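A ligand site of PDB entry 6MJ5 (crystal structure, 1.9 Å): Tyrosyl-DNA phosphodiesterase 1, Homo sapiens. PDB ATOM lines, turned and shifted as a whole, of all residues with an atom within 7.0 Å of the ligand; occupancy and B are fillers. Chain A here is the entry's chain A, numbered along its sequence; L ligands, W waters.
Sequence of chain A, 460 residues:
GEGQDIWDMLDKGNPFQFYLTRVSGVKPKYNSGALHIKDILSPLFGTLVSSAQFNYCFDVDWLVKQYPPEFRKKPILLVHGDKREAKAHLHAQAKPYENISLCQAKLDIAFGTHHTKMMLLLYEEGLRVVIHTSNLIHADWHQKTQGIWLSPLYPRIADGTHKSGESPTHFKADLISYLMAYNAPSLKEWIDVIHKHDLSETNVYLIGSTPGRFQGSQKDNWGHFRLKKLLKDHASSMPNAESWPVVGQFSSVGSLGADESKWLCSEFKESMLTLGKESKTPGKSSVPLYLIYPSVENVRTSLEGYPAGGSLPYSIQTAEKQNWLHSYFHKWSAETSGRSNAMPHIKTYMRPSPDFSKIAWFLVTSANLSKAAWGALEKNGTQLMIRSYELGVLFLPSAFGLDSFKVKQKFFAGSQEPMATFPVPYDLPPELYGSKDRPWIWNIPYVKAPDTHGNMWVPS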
ATOM      1  N   ASN A  55      27.057 -25.369 -35.991  1.00  0.00           N
ATOM      2  CA  ASN A  55      27.183 -25.600 -34.565  1.00  0.00           C
ATOM      3  C   ASN A  55      25.932 -25.132 -33.826  1.00  0.00           C
ATOM      4  O   ASN A  55      24.947 -24.674 -34.415  1.00  0.00           O
ATOM      5  CB  ASN A  55      28.449 -24.943 -33.997  1.00  0.00           C
ATOM      6  CG  ASN A  55      29.108 -25.817 -32.915  1.00  0.00           C
ATOM      7  OD1 ASN A  55      28.556 -25.958 -31.833  1.00  0.00           O
ATOM      8  ND2 ASN A  55      30.257 -26.413 -33.221  1.00  0.00           N
ATOM      9  N   TYR A  56      25.971 -25.297 -32.504  1.00  0.00           N
ATOM     10  CA  TYR A  56      24.905 -24.849 -31.624  1.00  0.00           C
ATOM     11  C   TYR A  56      25.246 -23.514 -30.970  1.00  0.00           C
ATOM     12  O   TYR A  56      24.511 -22.535 -31.114  1.00  0.00           O
ATOM     13  CB  TYR A  56      24.638 -25.926 -30.560  1.00  0.00           C
ATOM     14  CG  TYR A  56      23.676 -25.487 -29.494  1.00  0.00           C
ATOM     15  CD1 TYR A  56      22.323 -25.300 -29.796  1.00  0.00           C
ATOM     16  CD2 TYR A  56      24.123 -25.223 -28.197  1.00  0.00           C
ATOM     17  CE1 TYR A  56      21.444 -24.866 -28.821  1.00  0.00           C
ATOM     18  CE2 TYR A  56      23.240 -24.782 -27.229  1.00  0.00           C
ATOM     19  CZ  TYR A  56      21.910 -24.615 -27.534  1.00  0.00           C
ATOM     20  OH  TYR A  56      21.046 -24.195 -26.551  1.00  0.00           O
ATOM     21  N   CYS A  57      26.371 -23.466 -30.267  1.00  0.00           N
ATOM     22  CA  CYS A  57      26.794 -22.280 -29.542  1.00  0.00           C
ATOM     23  C   CYS A  57      28.085 -21.738 -30.155  1.00  0.00           C
ATOM     24  O   CYS A  57      28.993 -22.501 -30.479  1.00  0.00           O
ATOM     25  CB  CYS A  57      27.015 -22.624 -28.056  1.00  0.00           C
ATOM     26  SG  CYS A  57      27.248 -21.175 -27.038  1.00  0.00           S
ATOM     27  N   THR A 113      16.148 -27.962 -32.083  1.00  0.00           N
ATOM     28  CA  THR A 113      17.437 -27.308 -31.914  1.00  0.00           C
ATOM     29  C   THR A 113      18.349 -27.709 -33.056  1.00  0.00           C
ATOM     30  O   THR A 113      18.179 -28.769 -33.670  1.00  0.00           O
ATOM     31  CB  THR A 113      18.074 -27.724 -30.578  1.00  0.00           C
ATOM     32  OG1 THR A 113      17.980 -29.150 -30.495  1.00  0.00           O
ATOM     33  CG2 THR A 113      17.347 -27.118 -29.406  1.00  0.00           C
ATOM     34  N   HIS A 114      19.349 -26.871 -33.345  1.00  0.00           N
ATOM     35  CA  HIS A 114      20.386 -27.228 -34.315  1.00  0.00           C
ATOM     36  C   HIS A 114      21.633 -27.688 -33.556  1.00  0.00           C
ATOM     37  O   HIS A 114      22.451 -26.869 -33.136  1.00  0.00           O
ATOM     38  CB  HIS A 114      20.709 -26.060 -35.228  1.00  0.00           C
ATOM     39  CG  HIS A 114      21.687 -26.405 -36.304  1.00  0.00           C
ATOM     40  ND1 HIS A 114      23.040 -26.192 -36.165  1.00  0.00           N
ATOM     41  CD2 HIS A 114      21.515 -26.959 -37.530  1.00  0.00           C
ATOM     42  CE1 HIS A 114      23.671 -26.614 -37.253  1.00  0.00           C
ATOM     43  NE2 HIS A 114      22.767 -27.086 -38.095  1.00  0.00           N
ATOM     44  N   HIS A 115      21.773 -29.004 -33.384  1.00  0.00           N
ATOM     45  CA  HIS A 115      22.872 -29.559 -32.587  1.00  0.00           C
ATOM     46  C   HIS A 115      24.038 -30.066 -33.430  1.00  0.00           C
ATOM     47  O   HIS A 115      25.110 -30.344 -32.869  1.00  0.00           O
ATOM     48  CB  HIS A 115      22.370 -30.710 -31.702  1.00  0.00           C
ATOM     49  CG  HIS A 115      21.556 -30.253 -30.546  1.00  0.00           C
ATOM     50  ND1 HIS A 115      20.539 -31.016 -29.998  1.00  0.00           N
ATOM     51  CD2 HIS A 115      21.582 -29.100 -29.832  1.00  0.00           C
ATOM     52  CE1 HIS A 115      19.989 -30.359 -28.986  1.00  0.00           C
ATOM     53  NE2 HIS A 115      20.596 -29.187 -28.871  1.00  0.00           N
ATOM     54  N   THR A 116      23.878 -30.161 -34.752  1.00  0.00           N
ATOM     55  CA  THR A 116      24.930 -30.668 -35.629  1.00  0.00           C
ATOM     56  C   THR A 116      26.213 -29.856 -35.479  1.00  0.00           C
ATOM     57  O   THR A 116      26.181 -28.616 -35.502  1.00  0.00           O
ATOM     58  CB  THR A 116      24.454 -30.599 -37.072  1.00  0.00           C
ATOM     59  OG1 THR A 116      23.464 -31.609 -37.286  1.00  0.00           O
ATOM     60  CG2 THR A 116      25.621 -30.804 -38.029  1.00  0.00           C
ATOM     61  N   LYS A 117      27.337 -30.552 -35.345  1.00  0.00           N
ATOM     62  CA  LYS A 117      28.651 -29.927 -35.227  1.00  0.00           C
ATOM     63  C   LYS A 117      29.545 -30.453 -36.346  1.00  0.00           C
ATOM     64  O   LYS A 117      29.942 -31.624 -36.349  1.00  0.00           O
ATOM     65  CB  LYS A 117      29.212 -30.175 -33.841  1.00  0.00           C
ATOM     66  CG  LYS A 117      28.290 -29.494 -32.817  1.00  0.00           C
ATOM     67  CD  LYS A 117      28.789 -29.621 -31.412  1.00  0.00           C
ATOM     68  CE  LYS A 117      27.782 -28.974 -30.468  1.00  0.00           C
ATOM     69  NZ  LYS A 117      26.512 -29.730 -30.521  1.00  0.00           N
ATOM     70  N   THR A 133      31.965 -32.994 -31.842  1.00  0.00           N
ATOM     71  CA  THR A 133      30.965 -32.848 -30.799  1.00  0.00           C
ATOM     72  C   THR A 133      31.083 -31.561 -29.987  1.00  0.00           C
ATOM     73  O   THR A 133      30.276 -31.366 -29.066  1.00  0.00           O
ATOM     74  CB  THR A 133      31.022 -34.053 -29.832  1.00  0.00           C
ATOM     75  OG1 THR A 133      32.271 -34.065 -29.141  1.00  0.00           O
ATOM     76  CG2 THR A 133      30.900 -35.361 -30.582  1.00  0.00           C
ATOM     77  N   SER A 134      32.019 -30.669 -30.306  1.00  0.00           N
ATOM     78  CA  SER A 134      32.280 -29.493 -29.478  1.00  0.00           C
ATOM     79  C   SER A 134      31.568 -28.241 -29.995  1.00  0.00           C
ATOM     80  O   SER A 134      31.547 -27.973 -31.195  1.00  0.00           O
ATOM     81  CB  SER A 134      33.781 -29.181 -29.423  1.00  0.00           C
ATOM     82  OG  SER A 134      34.527 -30.293 -28.990  1.00  0.00           O
ATOM     83  N   ASN A 135      31.036 -27.455 -29.055  1.00  0.00           N
ATOM     84  CA  ASN A 135      30.615 -26.091 -29.378  1.00  0.00           C
ATOM     85  C   ASN A 135      31.837 -25.227 -29.678  1.00  0.00           C
ATOM     86  O   ASN A 135      32.976 -25.558 -29.328  1.00  0.00           O
ATOM     87  CB  ASN A 135      29.816 -25.490 -28.220  1.00  0.00           C
ATOM     88  CG  ASN A 135      28.486 -26.173 -28.039  1.00  0.00           C
ATOM     89  OD1 ASN A 135      27.528 -25.892 -28.767  1.00  0.00           O
ATOM     90  ND2 ASN A 135      28.425 -27.109 -27.090  1.00  0.00           N
ATOM     91  N   ASP A 140      34.516 -25.641 -24.306  1.00  0.00           N
ATOM     92  CA  ASP A 140      34.272 -26.954 -24.886  1.00  0.00           C
ATOM     93  C   ASP A 140      35.552 -27.613 -25.385  1.00  0.00           C
ATOM     94  O   ASP A 140      35.556 -28.833 -25.597  1.00  0.00           O
ATOM     95  CB  ASP A 140      33.224 -26.841 -26.017  1.00  0.00           C
ATOM     96  CG  ASP A 140      31.799 -27.177 -25.526  1.00  0.00           C
ATOM     97  OD1 ASP A 140      31.442 -26.742 -24.412  1.00  0.00           O
ATOM     98  OD2 ASP A 140      31.045 -27.900 -26.224  1.00  0.00           O
ATOM     99  N   SER A 251      25.590 -36.786 -22.890  1.00  0.00           N
ATOM    100  CA  SER A 251      25.772 -35.699 -21.940  1.00  0.00           C
ATOM    101  C   SER A 251      24.459 -35.073 -21.497  1.00  0.00           C
ATOM    102  O   SER A 251      24.474 -34.161 -20.653  1.00  0.00           O
ATOM    103  CB  SER A 251      26.702 -34.630 -22.548  1.00  0.00           C
ATOM    104  OG  SER A 251      26.131 -34.043 -23.686  1.00  0.00           O
ATOM    105  N   SER A 252      23.326 -35.546 -22.012  1.00  0.00           N
ATOM    106  CA  SER A 252      22.017 -35.008 -21.686  1.00  0.00           C
ATOM    107  C   SER A 252      20.983 -36.098 -21.924  1.00  0.00           C
ATOM    108  O   SER A 252      21.184 -36.987 -22.746  1.00  0.00           O
ATOM    109  CB  SER A 252      21.689 -33.760 -22.506  1.00  0.00           C
ATOM    110  OG  SER A 252      20.651 -33.019 -21.908  1.00  0.00           O
ATOM    111  N   GLY A 309      29.150 -29.252 -14.879  1.00  0.00           N
ATOM    112  CA  GLY A 309      27.738 -29.592 -14.937  1.00  0.00           C
ATOM    113  C   GLY A 309      26.898 -28.585 -15.691  1.00  0.00           C
ATOM    114  O   GLY A 309      25.747 -28.898 -16.026  1.00  0.00           O
ATOM    115  N   GLY A 310      27.447 -27.402 -15.960  1.00  0.00           N
ATOM    116  CA  GLY A 310      26.768 -26.451 -16.812  1.00  0.00           C
ATOM    117  C   GLY A 310      26.595 -26.952 -18.228  1.00  0.00           C
ATOM    118  O   GLY A 310      25.754 -26.424 -18.971  1.00  0.00           O
ATOM    119  N   SER A 311      27.357 -27.969 -18.634  1.00  0.00           N
ATOM    120  CA  SER A 311      27.241 -28.581 -19.951  1.00  0.00           C
ATOM    121  C   SER A 311      26.627 -29.971 -19.890  1.00  0.00           C
ATOM    122  O   SER A 311      26.778 -30.768 -20.824  1.00  0.00           O
ATOM    123  CB  SER A 311      28.601 -28.624 -20.644  1.00  0.00           C
ATOM    124  OG  SER A 311      29.079 -27.321 -20.890  1.00  0.00           O
ATOM    125  N   LEU A 312      25.930 -30.294 -18.815  1.00  0.00           N
ATOM    126  CA  LEU A 312      25.273 -31.597 -18.652  1.00  0.00           C
ATOM    127  C   LEU A 312      23.854 -31.274 -18.188  1.00  0.00           C
ATOM    128  O   LEU A 312      23.544 -31.412 -17.004  1.00  0.00           O
ATOM    129  CB  LEU A 312      26.019 -32.499 -17.656  1.00  0.00           C
ATOM    130  CG  LEU A 312      27.449 -32.978 -17.964  1.00  0.00           C
ATOM    131  CD1 LEU A 312      28.215 -33.327 -16.690  1.00  0.00           C
ATOM    132  CD2 LEU A 312      27.436 -34.182 -18.888  1.00  0.00           C
ATOM    133  N   PRO A 313      22.986 -30.803 -19.107  1.00  0.00           N
ATOM    134  CA  PRO A 313      21.757 -30.072 -18.720  1.00  0.00           C
ATOM    135  C   PRO A 313      20.551 -30.975 -18.444  1.00  0.00           C
ATOM    136  O   PRO A 313      19.481 -30.815 -19.036  1.00  0.00           O
ATOM    137  CB  PRO A 313      21.534 -29.157 -19.924  1.00  0.00           C
ATOM    138  CG  PRO A 313      22.052 -29.958 -21.100  1.00  0.00           C
ATOM    139  CD  PRO A 313      23.162 -30.856 -20.576  1.00  0.00           C
ATOM    140  N   HIS A 345      31.529 -34.473 -23.223  1.00  0.00           N
ATOM    141  CA  HIS A 345      30.547 -33.846 -24.082  1.00  0.00           C
ATOM    142  C   HIS A 345      30.433 -34.585 -25.407  1.00  0.00           C
ATOM    143  O   HIS A 345      29.544 -34.269 -26.218  1.00  0.00           O
ATOM    144  CB  HIS A 345      30.913 -32.371 -24.284  1.00  0.00           C
ATOM    145  CG  HIS A 345      29.847 -31.555 -24.956  1.00  0.00           C
ATOM    146  ND1 HIS A 345      29.870 -31.290 -26.308  1.00  0.00           N
ATOM    147  CD2 HIS A 345      28.754 -30.936 -24.465  1.00  0.00           C
ATOM    148  CE1 HIS A 345      28.823 -30.541 -26.628  1.00  0.00           C
ATOM    149  NE2 HIS A 345      28.126 -30.311 -25.521  1.00  0.00           N
ATOM    150  N   LYS A 347      29.215 -37.867 -27.488  1.00  0.00           N
ATOM    151  CA  LYS A 347      28.173 -38.870 -27.369  1.00  0.00           C
ATOM    152  C   LYS A 347      28.579 -40.036 -28.252  1.00  0.00           C
ATOM    153  O   LYS A 347      29.025 -39.835 -29.385  1.00  0.00           O
ATOM    154  CB  LYS A 347      26.775 -38.381 -27.811  1.00  0.00           C
ATOM    155  CG  LYS A 347      26.258 -37.194 -27.024  1.00  0.00           C
ATOM    156  CD  LYS A 347      26.668 -35.878 -27.697  1.00  0.00           C
ATOM    157  CE  LYS A 347      25.994 -34.701 -27.019  1.00  0.00           C
ATOM    158  NZ  LYS A 347      26.940 -33.570 -26.848  1.00  0.00           N
ATOM    159  N   SER A 366      26.472 -36.036 -32.378  1.00  0.00           N
ATOM    160  CA  SER A 366      25.940 -34.986 -31.514  1.00  0.00           C
ATOM    161  C   SER A 366      24.649 -35.404 -30.793  1.00  0.00           C
ATOM    162  O   SER A 366      24.220 -34.691 -29.887  1.00  0.00           O
ATOM    163  CB  SER A 366      25.697 -33.710 -32.333  1.00  0.00           C
ATOM    164  OG  SER A 366      24.726 -33.942 -33.363  1.00  0.00           O
ATOM    165  N   ASN A 368      22.155 -36.755 -28.265  1.00  0.00           N
ATOM    166  CA  ASN A 368      21.952 -37.200 -26.898  1.00  0.00           C
ATOM    167  C   ASN A 368      20.849 -38.260 -26.833  1.00  0.00           C
ATOM    168  O   ASN A 368      20.256 -38.655 -27.847  1.00  0.00           O
ATOM    169  CB  ASN A 368      21.655 -36.005 -26.008  1.00  0.00           C
ATOM    170  CG  ASN A 368      22.913 -35.331 -25.552  1.00  0.00           C
ATOM    171  OD1 ASN A 368      23.855 -35.994 -25.095  1.00  0.00           O
ATOM    172  ND2 ASN A 368      22.988 -34.012 -25.711  1.00  0.00           N
ATOM    173  N   GLU A 390      20.925 -33.220 -36.117  1.00  0.00           N
ATOM    174  CA  GLU A 390      22.025 -33.951 -35.494  1.00  0.00           C
ATOM    175  C   GLU A 390      22.847 -34.613 -36.588  1.00  0.00           C
ATOM    176  O   GLU A 390      22.355 -34.834 -37.699  1.00  0.00           O
ATOM    177  CB  GLU A 390      21.578 -35.063 -34.522  1.00  0.00           C
ATOM    178  CG  GLU A 390      20.460 -34.712 -33.563  1.00  0.00           C
ATOM    179  CD  GLU A 390      20.954 -33.999 -32.307  1.00  0.00           C
ATOM    180  OE1 GLU A 390      20.113 -33.450 -31.537  1.00  0.00           O
ATOM    181  OE2 GLU A 390      22.175 -33.947 -32.088  1.00  0.00           O
ATOM    182  N   TRP A 442      21.500 -30.610 -13.188  1.00  0.00           N
ATOM    183  CA  TRP A 442      22.212 -29.339 -13.183  1.00  0.00           C
ATOM    184  C   TRP A 442      21.490 -28.223 -12.433  1.00  0.00           C
ATOM    185  O   TRP A 442      22.151 -27.240 -12.074  1.00  0.00           O
ATOM    186  CB  TRP A 442      22.513 -28.844 -14.614  1.00  0.00           C
ATOM    187  CG  TRP A 442      21.368 -28.321 -15.423  1.00  0.00           C
ATOM    188  CD1 TRP A 442      20.051 -28.682 -15.322  1.00  0.00           C
ATOM    189  CD2 TRP A 442      21.447 -27.371 -16.504  1.00  0.00           C
ATOM    190  NE1 TRP A 442      19.302 -27.993 -16.259  1.00  0.00           N
ATOM    191  CE2 TRP A 442      20.142 -27.190 -16.998  1.00  0.00           C
ATOM    192  CE3 TRP A 442      22.495 -26.651 -17.092  1.00  0.00           C
ATOM    193  CZ2 TRP A 442      19.847 -26.310 -18.048  1.00  0.00           C
ATOM    194  CZ3 TRP A 442      22.204 -25.778 -18.136  1.00  0.00           C
ATOM    195  CH2 TRP A 442      20.891 -25.622 -18.605  1.00  0.00           C
HETATM  196  C1  LIG L   1      24.130 -26.730 -21.761  1.00  0.00           C
HETATM  197  C2  LIG L   1      24.237 -27.544 -24.057  1.00  0.00           C
HETATM  198  C3  LIG L   1      25.036 -28.962 -27.502  1.00  0.00           C
HETATM  199  C4  LIG L   1      24.308 -28.352 -26.305  1.00  0.00           C
HETATM  200  C5  LIG L   1      22.965 -28.011 -26.416  1.00  0.00           C
HETATM  201  C6  LIG L   1      22.910 -27.238 -24.239  1.00  0.00           C
HETATM  202  C7  LIG L   1      22.174 -26.666 -23.173  1.00  0.00           C
HETATM  203  C8  LIG L   1      22.787 -26.410 -21.951  1.00  0.00           C
HETATM  204  C9  LIG L   1      24.859 -27.296 -22.816  1.00  0.00           C
HETATM  205  C10 LIG L   1      24.960 -28.119 -25.102  1.00  0.00           C
HETATM  206  N1  LIG L   1      22.297 -27.478 -25.406  1.00  0.00           N
HETATM  207  N2  LIG L   1      20.778 -26.323 -23.354  1.00  0.00           N
HETATM  208  O1  LIG L   1      24.367 -29.359 -28.490  1.00  0.00           O
HETATM  209  O2  LIG L   1      26.285 -29.029 -27.504  1.00  0.00           O
HETATM  210  O3  LIG L   1      20.025 -27.113 -23.793  1.00  0.00           O
HETATM  211  O4  LIG L   1      20.411 -25.239 -23.081  1.00  0.00           O
HETATM  212  O5  LIG L   1      26.312 -28.438 -24.916  1.00  0.00           O
HETATM  213  O   HOH W   1      19.693 -27.683 -26.569  1.00  0.00           O
HETATM  214  O   HOH W   2      28.737 -26.981 -23.656  1.00  0.00           O
HETATM  215  O   HOH W   3      22.669 -31.556 -27.396  1.00  0.00           O
HETATM  216  O   HOH W   4      24.822 -32.018 -28.908  1.00  0.00           O
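CE2 of Tyr 56 touches C5 of the ligand (3.3 Å). CD2 of His 115 touches O1 of the ligand, 3.1 Å away. Gly 310 touches the ligand (O to C1, 3.2 Å). Ser 311 touches the ligand (CA to C9, 3.9 Å). Pro 313 touches the ligand (CB to C8, 3.6 Å). Trp 442 touches the ligand (CZ3 to C8, 3.9 Å). Hydrophobic or aromatic side chains within 4 Å of the ligand: Tyr 56, His 115, Pro 313, His 345 and Trp 442. Of the 25 residues printed, 9 come within 4 Å of the ligand. Along chain A the residues within 4 Å of the ligand span positions 56 to 442. The nearest printed residue that does not touch the ligand is Lys 347 (4.6 Å).
OD1 of Asn 135 sits close to OD1 of Asn 55 (3.2 Å). The backbone NH (N) of Asn 135 lies within hydrogen-bond range of the side-chain carboxylate (OD2) of Asp 140. The side-chain amino group of Lys 347 sits at hydrogen-bond distance from the backbone carbonyl oxygen of His 345. ND1 of His 345 lies within hydrogen-bond range of O of Thr 133, 2.8 Å away. A ring nitrogen (NE2) of His 115 sits close to the side-chain hydroxyl (OG1) of Thr 113 (3.1 Å). ND1 of His 115 is in hydrogen-bond range of OE1 of Glu 390 (2.9 Å). The side-chain amino group of Lys 117 lies within hydrogen-bond range of the backbone carbonyl oxygen of His 115 (2.8 Å). The backbone NH (N) of Cys 57 is in hydrogen-bond range of the side-chain amide oxygen (OD1) of Asn 135 (3.1 Å).
Water W4 lies within hydrogen-bond range of an oxygen (O1) of the ligand, the backbone carbonyl oxygen of Ser 366, the side-chain amino group of Lys 117 and the side-chain amino group of Lys 347. Water W1 bridges an oxygen (O3) of the ligand (2.9 Å) and a ring nitrogen (NE2) of His 115 (2.9 Å). Water W3 lies within hydrogen-bond range of an oxygen (O1) of the ligand, the side-chain amide nitrogen (ND2) of Asn 368 and a ring nitrogen (ND1) of His 115. Water W2 lies within hydrogen-bond range of OG of Ser 311, OD1 of Asp 140, O5 of the ligand and ND2 of Asn 135.
NE2 of His 345 lies within hydrogen-bond range of O5 of the ligand (2.7 Å). The side-chain amide nitrogen of Asn 135 lies within hydrogen-bond range of an oxygen (O2) of the ligand (2.9 Å). The side-chain amino group (NZ) of Lys 117 lies within salt-bridge range of an oxygen (O1) of the ligand (3.0 Å).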
